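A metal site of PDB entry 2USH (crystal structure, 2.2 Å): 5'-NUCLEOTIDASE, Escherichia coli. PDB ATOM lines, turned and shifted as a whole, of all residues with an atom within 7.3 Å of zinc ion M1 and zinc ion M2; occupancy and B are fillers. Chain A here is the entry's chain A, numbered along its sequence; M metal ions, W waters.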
ATOM      1  N   ASN A  40      18.524 -15.205  -9.116  1.00  0.00           N
ATOM      2  CA  ASN A  40      19.665 -14.819  -8.288  1.00  0.00           C
ATOM      3  C   ASN A  40      20.676 -14.039  -9.093  1.00  0.00           C
ATOM      4  O   ASN A  40      20.657 -14.085 -10.311  1.00  0.00           O
ATOM      5  CB  ASN A  40      20.374 -16.054  -7.717  1.00  0.00           C
ATOM      6  CG  ASN A  40      20.770 -17.019  -8.795  1.00  0.00           C
ATOM      7  OD1 ASN A  40      19.925 -17.763  -9.327  1.00  0.00           O
ATOM      8  ND2 ASN A  40      22.050 -17.006  -9.152  1.00  0.00           N
ATOM      9  N   ASP A  41      21.543 -13.310  -8.399  1.00  0.00           N
ATOM     10  CA  ASP A  41      22.614 -12.567  -9.053  1.00  0.00           C
ATOM     11  C   ASP A  41      22.171 -11.720 -10.235  1.00  0.00           C
ATOM     12  O   ASP A  41      22.729 -11.800 -11.335  1.00  0.00           O
ATOM     13  CB  ASP A  41      23.662 -13.577  -9.447  1.00  0.00           C
ATOM     14  CG  ASP A  41      24.162 -14.321  -8.239  1.00  0.00           C
ATOM     15  OD1 ASP A  41      23.571 -15.358  -7.854  1.00  0.00           O
ATOM     16  OD2 ASP A  41      25.125 -13.807  -7.645  1.00  0.00           O
ATOM     17  N   HIS A  42      21.152 -10.920  -9.944  1.00  0.00           N
ATOM     18  CA  HIS A  42      20.514  -9.961 -10.830  1.00  0.00           C
ATOM     19  C   HIS A  42      21.550  -8.950 -11.317  1.00  0.00           C
ATOM     20  O   HIS A  42      21.585  -8.600 -12.491  1.00  0.00           O
ATOM     21  CB  HIS A  42      19.386  -9.254 -10.061  1.00  0.00           C
ATOM     22  CG  HIS A  42      18.703  -8.182 -10.857  1.00  0.00           C
ATOM     23  ND1 HIS A  42      17.947  -8.467 -11.965  1.00  0.00           N
ATOM     24  CD2 HIS A  42      18.746  -6.837 -10.742  1.00  0.00           C
ATOM     25  CE1 HIS A  42      17.549  -7.332 -12.518  1.00  0.00           C
ATOM     26  NE2 HIS A  42      18.026  -6.328 -11.799  1.00  0.00           N
ATOM     27  N   HIS A  43      22.379  -8.481 -10.390  1.00  0.00           N
ATOM     28  CA  HIS A  43      23.446  -7.545 -10.705  1.00  0.00           C
ATOM     29  C   HIS A  43      23.217  -6.320 -11.615  1.00  0.00           C
ATOM     30  O   HIS A  43      23.970  -6.093 -12.542  1.00  0.00           O
ATOM     31  CB  HIS A  43      24.685  -8.325 -11.199  1.00  0.00           C
ATOM     32  CG  HIS A  43      25.366  -9.122 -10.121  1.00  0.00           C
ATOM     33  ND1 HIS A  43      25.783  -8.556  -8.936  1.00  0.00           N
ATOM     34  CD2 HIS A  43      25.743 -10.417 -10.066  1.00  0.00           C
ATOM     35  CE1 HIS A  43      26.388  -9.461  -8.200  1.00  0.00           C
ATOM     36  NE2 HIS A  43      26.371 -10.610  -8.855  1.00  0.00           N
ATOM     37  N   GLY A  82      17.989 -15.272  -4.722  1.00  0.00           N
ATOM     38  CA  GLY A  82      19.215 -15.704  -4.065  1.00  0.00           C
ATOM     39  C   GLY A  82      20.214 -14.567  -3.807  1.00  0.00           C
ATOM     40  O   GLY A  82      21.384 -14.838  -3.487  1.00  0.00           O
ATOM     41  N   GLY A  83      19.806 -13.304  -3.965  1.00  0.00           N
ATOM     42  CA  GLY A  83      20.722 -12.210  -3.679  1.00  0.00           C
ATOM     43  C   GLY A  83      21.575 -11.650  -4.810  1.00  0.00           C
ATOM     44  O   GLY A  83      21.509 -12.140  -5.938  1.00  0.00           O
ATOM     45  N   ASP A  84      22.449 -10.699  -4.475  1.00  0.00           N
ATOM     46  CA  ASP A  84      23.280  -9.968  -5.454  1.00  0.00           C
ATOM     47  C   ASP A  84      22.460  -9.202  -6.497  1.00  0.00           C
ATOM     48  O   ASP A  84      22.490  -9.490  -7.686  1.00  0.00           O
ATOM     49  CB  ASP A  84      24.323 -10.852  -6.134  1.00  0.00           C
ATOM     50  CG  ASP A  84      25.572 -11.025  -5.298  1.00  0.00           C
ATOM     51  OD1 ASP A  84      25.647 -10.417  -4.218  1.00  0.00           O
ATOM     52  OD2 ASP A  84      26.503 -11.730  -5.722  1.00  0.00           O
ATOM     53  N   ILE A  85      21.717  -8.217  -6.008  1.00  0.00           N
ATOM     54  CA  ILE A  85      20.887  -7.372  -6.833  1.00  0.00           C
ATOM     55  C   ILE A  85      21.808  -6.231  -7.256  1.00  0.00           C
ATOM     56  O   ILE A  85      21.714  -5.711  -8.367  1.00  0.00           O
ATOM     57  CB  ILE A  85      19.708  -6.795  -5.989  1.00  0.00           C
ATOM     58  CG1 ILE A  85      18.992  -7.961  -5.306  1.00  0.00           C
ATOM     59  CG2 ILE A  85      18.777  -5.949  -6.854  1.00  0.00           C
ATOM     60  CD1 ILE A  85      18.531  -9.049  -6.237  1.00  0.00           C
ATOM     61  N   ASN A  86      22.700  -5.848  -6.341  1.00  0.00           N
ATOM     62  CA  ASN A  86      23.692  -4.792  -6.522  1.00  0.00           C
ATOM     63  C   ASN A  86      24.884  -5.152  -7.383  1.00  0.00           C
ATOM     64  O   ASN A  86      25.322  -6.303  -7.418  1.00  0.00           O
ATOM     65  CB  ASN A  86      24.276  -4.315  -5.164  1.00  0.00           C
ATOM     66  CG  ASN A  86      23.308  -3.458  -4.344  1.00  0.00           C
ATOM     67  OD1 ASN A  86      23.270  -2.245  -4.513  1.00  0.00           O
ATOM     68  ND2 ASN A  86      22.562  -4.060  -3.426  1.00  0.00           N
ATOM     69  N   THR A  87      25.410  -4.125  -8.051  1.00  0.00           N
ATOM     70  CA  THR A  87      26.650  -4.187  -8.839  1.00  0.00           C
ATOM     71  C   THR A  87      26.652  -4.962 -10.135  1.00  0.00           C
ATOM     72  O   THR A  87      26.467  -6.156 -10.133  1.00  0.00           O
ATOM     73  CB  THR A  87      27.760  -4.745  -7.966  1.00  0.00           C
ATOM     74  OG1 THR A  87      27.834  -3.960  -6.755  1.00  0.00           O
ATOM     75  CG2 THR A  87      29.104  -4.698  -8.689  1.00  0.00           C
ATOM     76  N   GLY A 115      23.143 -11.000  -0.550  1.00  0.00           N
ATOM     77  CA  GLY A 115      24.359 -11.464  -1.201  1.00  0.00           C
ATOM     78  C   GLY A 115      25.622 -10.714  -0.800  1.00  0.00           C
ATOM     79  O   GLY A 115      25.576  -9.705  -0.105  1.00  0.00           O
ATOM     80  N   ASN A 116      26.779 -11.203  -1.232  1.00  0.00           N
ATOM     81  CA  ASN A 116      28.001 -10.533  -0.875  1.00  0.00           C
ATOM     82  C   ASN A 116      28.074  -9.128  -1.490  1.00  0.00           C
ATOM     83  O   ASN A 116      28.633  -8.221  -0.891  1.00  0.00           O
ATOM     84  CB  ASN A 116      29.216 -11.405  -1.256  1.00  0.00           C
ATOM     85  CG  ASN A 116      29.286 -11.694  -2.741  1.00  0.00           C
ATOM     86  OD1 ASN A 116      28.333 -12.164  -3.344  1.00  0.00           O
ATOM     87  ND2 ASN A 116      30.445 -11.429  -3.342  1.00  0.00           N
ATOM     88  N   HIS A 117      27.496  -8.934  -2.669  1.00  0.00           N
ATOM     89  CA  HIS A 117      27.529  -7.602  -3.284  1.00  0.00           C
ATOM     90  C   HIS A 117      26.536  -6.558  -2.743  1.00  0.00           C
ATOM     91  O   HIS A 117      26.465  -5.443  -3.280  1.00  0.00           O
ATOM     92  CB  HIS A 117      27.428  -7.665  -4.826  1.00  0.00           C
ATOM     93  CG  HIS A 117      28.671  -8.194  -5.479  1.00  0.00           C
ATOM     94  ND1 HIS A 117      29.775  -7.399  -5.715  1.00  0.00           N
ATOM     95  CD2 HIS A 117      29.026  -9.448  -5.862  1.00  0.00           C
ATOM     96  CE1 HIS A 117      30.762  -8.137  -6.185  1.00  0.00           C
ATOM     97  NE2 HIS A 117      30.332  -9.376  -6.289  1.00  0.00           N
ATOM     98  N   THR A 172      27.120 -15.995   2.259  1.00  0.00           N
ATOM     99  CA  THR A 172      28.497 -16.503   2.259  1.00  0.00           C
ATOM    100  C   THR A 172      29.386 -15.704   3.198  1.00  0.00           C
ATOM    101  O   THR A 172      29.368 -14.470   3.229  1.00  0.00           O
ATOM    102  CB  THR A 172      29.149 -16.488   0.831  1.00  0.00           C
ATOM    103  OG1 THR A 172      30.478 -17.014   0.930  1.00  0.00           O
ATOM    104  CG2 THR A 172      29.202 -15.084   0.257  1.00  0.00           C
ATOM    105  N   THR A 175      32.169 -12.967   2.130  1.00  0.00           N
ATOM    106  CA  THR A 175      31.859 -11.581   1.871  1.00  0.00           C
ATOM    107  C   THR A 175      32.923 -10.656   2.389  1.00  0.00           C
ATOM    108  O   THR A 175      33.203  -9.674   1.747  1.00  0.00           O
ATOM    109  CB  THR A 175      30.488 -11.224   2.448  1.00  0.00           C
ATOM    110  OG1 THR A 175      29.504 -11.999   1.747  1.00  0.00           O
ATOM    111  CG2 THR A 175      30.193  -9.709   2.292  1.00  0.00           C
ATOM    112  N   HIS A 217      23.051 -17.387  -0.358  1.00  0.00           N
ATOM    113  CA  HIS A 217      23.960 -16.806  -1.334  1.00  0.00           C
ATOM    114  C   HIS A 217      25.347 -17.379  -0.996  1.00  0.00           C
ATOM    115  O   HIS A 217      26.219 -16.687  -0.473  1.00  0.00           O
ATOM    116  CB  HIS A 217      23.929 -15.303  -1.238  1.00  0.00           C
ATOM    117  CG  HIS A 217      24.614 -14.662  -2.380  1.00  0.00           C
ATOM    118  ND1 HIS A 217      23.956 -14.425  -3.566  1.00  0.00           N
ATOM    119  CD2 HIS A 217      25.910 -14.347  -2.583  1.00  0.00           C
ATOM    120  CE1 HIS A 217      24.829 -14.000  -4.459  1.00  0.00           C
ATOM    121  NE2 HIS A 217      26.023 -13.958  -3.892  1.00  0.00           N
ATOM    122  N   MET A 218      25.527 -18.667  -1.320  1.00  0.00           N
ATOM    123  CA  MET A 218      26.748 -19.398  -0.959  1.00  0.00           C
ATOM    124  C   MET A 218      27.479 -20.095  -2.113  1.00  0.00           C
ATOM    125  O   MET A 218      28.684 -20.283  -2.041  1.00  0.00           O
ATOM    126  CB  MET A 218      26.377 -20.394   0.160  1.00  0.00           C
ATOM    127  CG  MET A 218      25.798 -19.690   1.429  1.00  0.00           C
ATOM    128  SD  MET A 218      25.028 -20.797   2.648  1.00  0.00           S
ATOM    129  CE  MET A 218      26.104 -22.236   2.618  1.00  0.00           C
ATOM    130  N   GLY A 251      22.636 -19.131  -5.094  1.00  0.00           N
ATOM    131  CA  GLY A 251      23.227 -18.083  -5.918  1.00  0.00           C
ATOM    132  C   GLY A 251      24.724 -17.974  -5.691  1.00  0.00           C
ATOM    133  O   GLY A 251      25.364 -18.919  -5.208  1.00  0.00           O
ATOM    134  N   HIS A 252      25.285 -16.841  -6.079  1.00  0.00           N
ATOM    135  CA  HIS A 252      26.685 -16.525  -5.870  1.00  0.00           C
ATOM    136  C   HIS A 252      27.652 -17.143  -6.857  1.00  0.00           C
ATOM    137  O   HIS A 252      28.454 -16.434  -7.463  1.00  0.00           O
ATOM    138  CB  HIS A 252      27.115 -16.889  -4.438  1.00  0.00           C
ATOM    139  CG  HIS A 252      28.504 -16.428  -4.096  1.00  0.00           C
ATOM    140  ND1 HIS A 252      28.896 -15.121  -4.236  1.00  0.00           N
ATOM    141  CD2 HIS A 252      29.577 -17.098  -3.621  1.00  0.00           C
ATOM    142  CE1 HIS A 252      30.156 -15.001  -3.866  1.00  0.00           C
ATOM    143  NE2 HIS A 252      30.591 -16.178  -3.492  1.00  0.00           N
ATOM    144  N   SER A 253      27.622 -18.461  -6.981  1.00  0.00           N
ATOM    145  CA  SER A 253      28.480 -19.126  -7.948  1.00  0.00           C
ATOM    146  C   SER A 253      27.987 -18.770  -9.363  1.00  0.00           C
ATOM    147  O   SER A 253      28.751 -18.813 -10.296  1.00  0.00           O
ATOM    148  CB  SER A 253      28.500 -20.654  -7.735  1.00  0.00           C
ATOM    149  OG  SER A 253      27.219 -21.271  -7.819  1.00  0.00           O
ATOM    150  N   GLN A 254      26.700 -18.426  -9.503  1.00  0.00           N
ATOM    151  CA  GLN A 254      26.094 -18.047 -10.770  1.00  0.00           C
ATOM    152  C   GLN A 254      26.099 -19.074 -11.880  1.00  0.00           C
ATOM    153  O   GLN A 254      26.512 -18.796 -13.001  1.00  0.00           O
ATOM    154  CB  GLN A 254      26.699 -16.731 -11.265  1.00  0.00           C
ATOM    155  CG  GLN A 254      26.448 -15.612 -10.263  1.00  0.00           C
ATOM    156  CD  GLN A 254      27.066 -14.290 -10.673  1.00  0.00           C
ATOM    157  OE1 GLN A 254      27.466 -13.490  -9.825  1.00  0.00           O
ATOM    158  NE2 GLN A 254      27.128 -14.047 -11.982  1.00  0.00           N
ATOM    159  N   HIS A 289      21.467 -19.296 -12.526  1.00  0.00           N
ATOM    160  CA  HIS A 289      22.510 -18.640 -13.264  1.00  0.00           C
ATOM    161  C   HIS A 289      22.727 -17.167 -12.875  1.00  0.00           C
ATOM    162  O   HIS A 289      23.289 -16.892 -11.812  1.00  0.00           O
ATOM    163  CB  HIS A 289      22.173 -18.778 -14.746  1.00  0.00           C
ATOM    164  CG  HIS A 289      23.257 -18.329 -15.656  1.00  0.00           C
ATOM    165  ND1 HIS A 289      24.589 -18.432 -15.329  1.00  0.00           N
ATOM    166  CD2 HIS A 289      23.213 -17.816 -16.912  1.00  0.00           C
ATOM    167  CE1 HIS A 289      25.327 -18.006 -16.346  1.00  0.00           C
ATOM    168  NE2 HIS A 289      24.509 -17.636 -17.317  1.00  0.00           N
ATOM    169  N   GLU A 290      22.298 -16.203 -13.684  1.00  0.00           N
ATOM    170  CA  GLU A 290      22.565 -14.832 -13.305  1.00  0.00           C
ATOM    171  C   GLU A 290      21.820 -13.879 -14.229  1.00  0.00           C
ATOM    172  O   GLU A 290      21.309 -14.288 -15.259  1.00  0.00           O
ATOM    173  CB  GLU A 290      24.069 -14.537 -13.490  1.00  0.00           C
ATOM    174  CG  GLU A 290      24.402 -14.535 -14.996  1.00  0.00           C
ATOM    175  CD  GLU A 290      25.869 -14.577 -15.323  1.00  0.00           C
ATOM    176  OE1 GLU A 290      26.693 -14.786 -14.413  1.00  0.00           O
ATOM    177  OE2 GLU A 290      26.188 -14.418 -16.512  1.00  0.00           O
ATOM    178  N   TRP A 291      21.802 -12.597 -13.815  1.00  0.00           N
ATOM    179  CA  TRP A 291      21.250 -11.473 -14.578  1.00  0.00           C
ATOM    180  C   TRP A 291      19.804 -11.464 -15.077  1.00  0.00           C
ATOM    181  O   TRP A 291      19.486 -10.722 -16.010  1.00  0.00           O
ATOM    182  CB  TRP A 291      22.144 -11.215 -15.804  1.00  0.00           C
ATOM    183  CG  TRP A 291      23.606 -10.973 -15.482  1.00  0.00           C
ATOM    184  CD1 TRP A 291      24.185 -10.871 -14.247  1.00  0.00           C
ATOM    185  CD2 TRP A 291      24.679 -10.852 -16.446  1.00  0.00           C
ATOM    186  NE1 TRP A 291      25.543 -10.692 -14.376  1.00  0.00           N
ATOM    187  CE2 TRP A 291      25.869 -10.678 -15.712  1.00  0.00           C
ATOM    188  CE3 TRP A 291      24.741 -10.872 -17.853  1.00  0.00           C
ATOM    189  CZ2 TRP A 291      27.131 -10.525 -16.344  1.00  0.00           C
ATOM    190  CZ3 TRP A 291      25.986 -10.717 -18.480  1.00  0.00           C
ATOM    191  CH2 TRP A 291      27.166 -10.542 -17.714  1.00  0.00           C
ATOM    192  N   THR A 518      35.656 -11.819  -8.817  1.00  0.00           N
ATOM    193  CA  THR A 518      35.167 -10.797  -7.867  1.00  0.00           C
ATOM    194  C   THR A 518      33.784 -10.274  -8.164  1.00  0.00           C
ATOM    195  O   THR A 518      33.145  -9.704  -7.302  1.00  0.00           O
ATOM    196  CB  THR A 518      36.063  -9.567  -7.819  1.00  0.00           C
ATOM    197  OG1 THR A 518      36.029  -8.919  -9.109  1.00  0.00           O
ATOM    198  CG2 THR A 518      37.496  -9.964  -7.486  1.00  0.00           C
ATOM    199  N   GLY A 519      33.319 -10.450  -9.388  1.00  0.00           N
ATOM    200  CA  GLY A 519      32.023  -9.898  -9.693  1.00  0.00           C
ATOM    201  C   GLY A 519      32.122  -8.394  -9.967  1.00  0.00           C
ATOM    202  O   GLY A 519      31.096  -7.773 -10.194  1.00  0.00           O
HETATM  203 ZN    ZN M   1      27.758 -13.366  -4.820  1.00  0.00          ZN
HETATM  204 ZN    ZN M   2      26.782 -12.519  -7.889  1.00  0.00          ZN
HETATM  205  O   HOH W   1      28.365 -13.310  -6.864  1.00  0.00           O
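O of Gly 83 lies within hydrogen-bond range of N of Asp 41 (2.7 Å). The backbone NH (N) of His 43 lies close to the backbone carbonyl oxygen (O) of Ile 85 (3.5 Å). The side-chain carboxylate of Asp 41 lies within hydrogen-bond range of the side-chain amide nitrogen of Asn 40, 2.6 Å away. A ring nitrogen (ND1) of His 43 is in hydrogen-bond range of the backbone carbonyl oxygen (O) of Asn 86, at 2.8 Å. The side-chain carboxylate of Asp 84 is in hydrogen-bond range of the backbone NH of His 117 (2.8 Å). The side-chain amide nitrogen of Gln 254 is in hydrogen-bond range of the side-chain carboxylate of Glu 290 (2.6 Å). The backbone carbonyl oxygen (O) of Gly 82 is in hydrogen-bond range of a ring nitrogen (ND1) of His 217, 2.6 Å away. O of Asp 84 sits at hydrogen-bond distance from N of His 42 (3.0 Å).
Of the 26 residues printed, 5 come within 4 Å of zinc ion M1.
Zinc ion M1 is bound by the side-chain amide oxygen of Asn 116 (2.0 Å), a ring nitrogen (NE2) of His 217 (2.1 Å), water W1 (2.1 Å), a ring nitrogen (ND1) of His 252 (2.2 Å) and the side-chain carboxylate of Asp 84 (2.3 Å).
Zinc ion M2 is bound by water W1, the side-chain carboxylate of Asp 41, a ring nitrogen (NE2) of His 43, the side-chain amide oxygen of Gln 254 and the side-chain carboxylate of Asp 84. Zinc ion M2 has five donor atoms within binding distance.
Four residues have an atom within 4 Å of zinc ion M2: Asp 41, His 43, Asp 84 and Gln 254. The nearest printed residue that does not touch zinc ion M2 is His 217 (4.2 Å).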
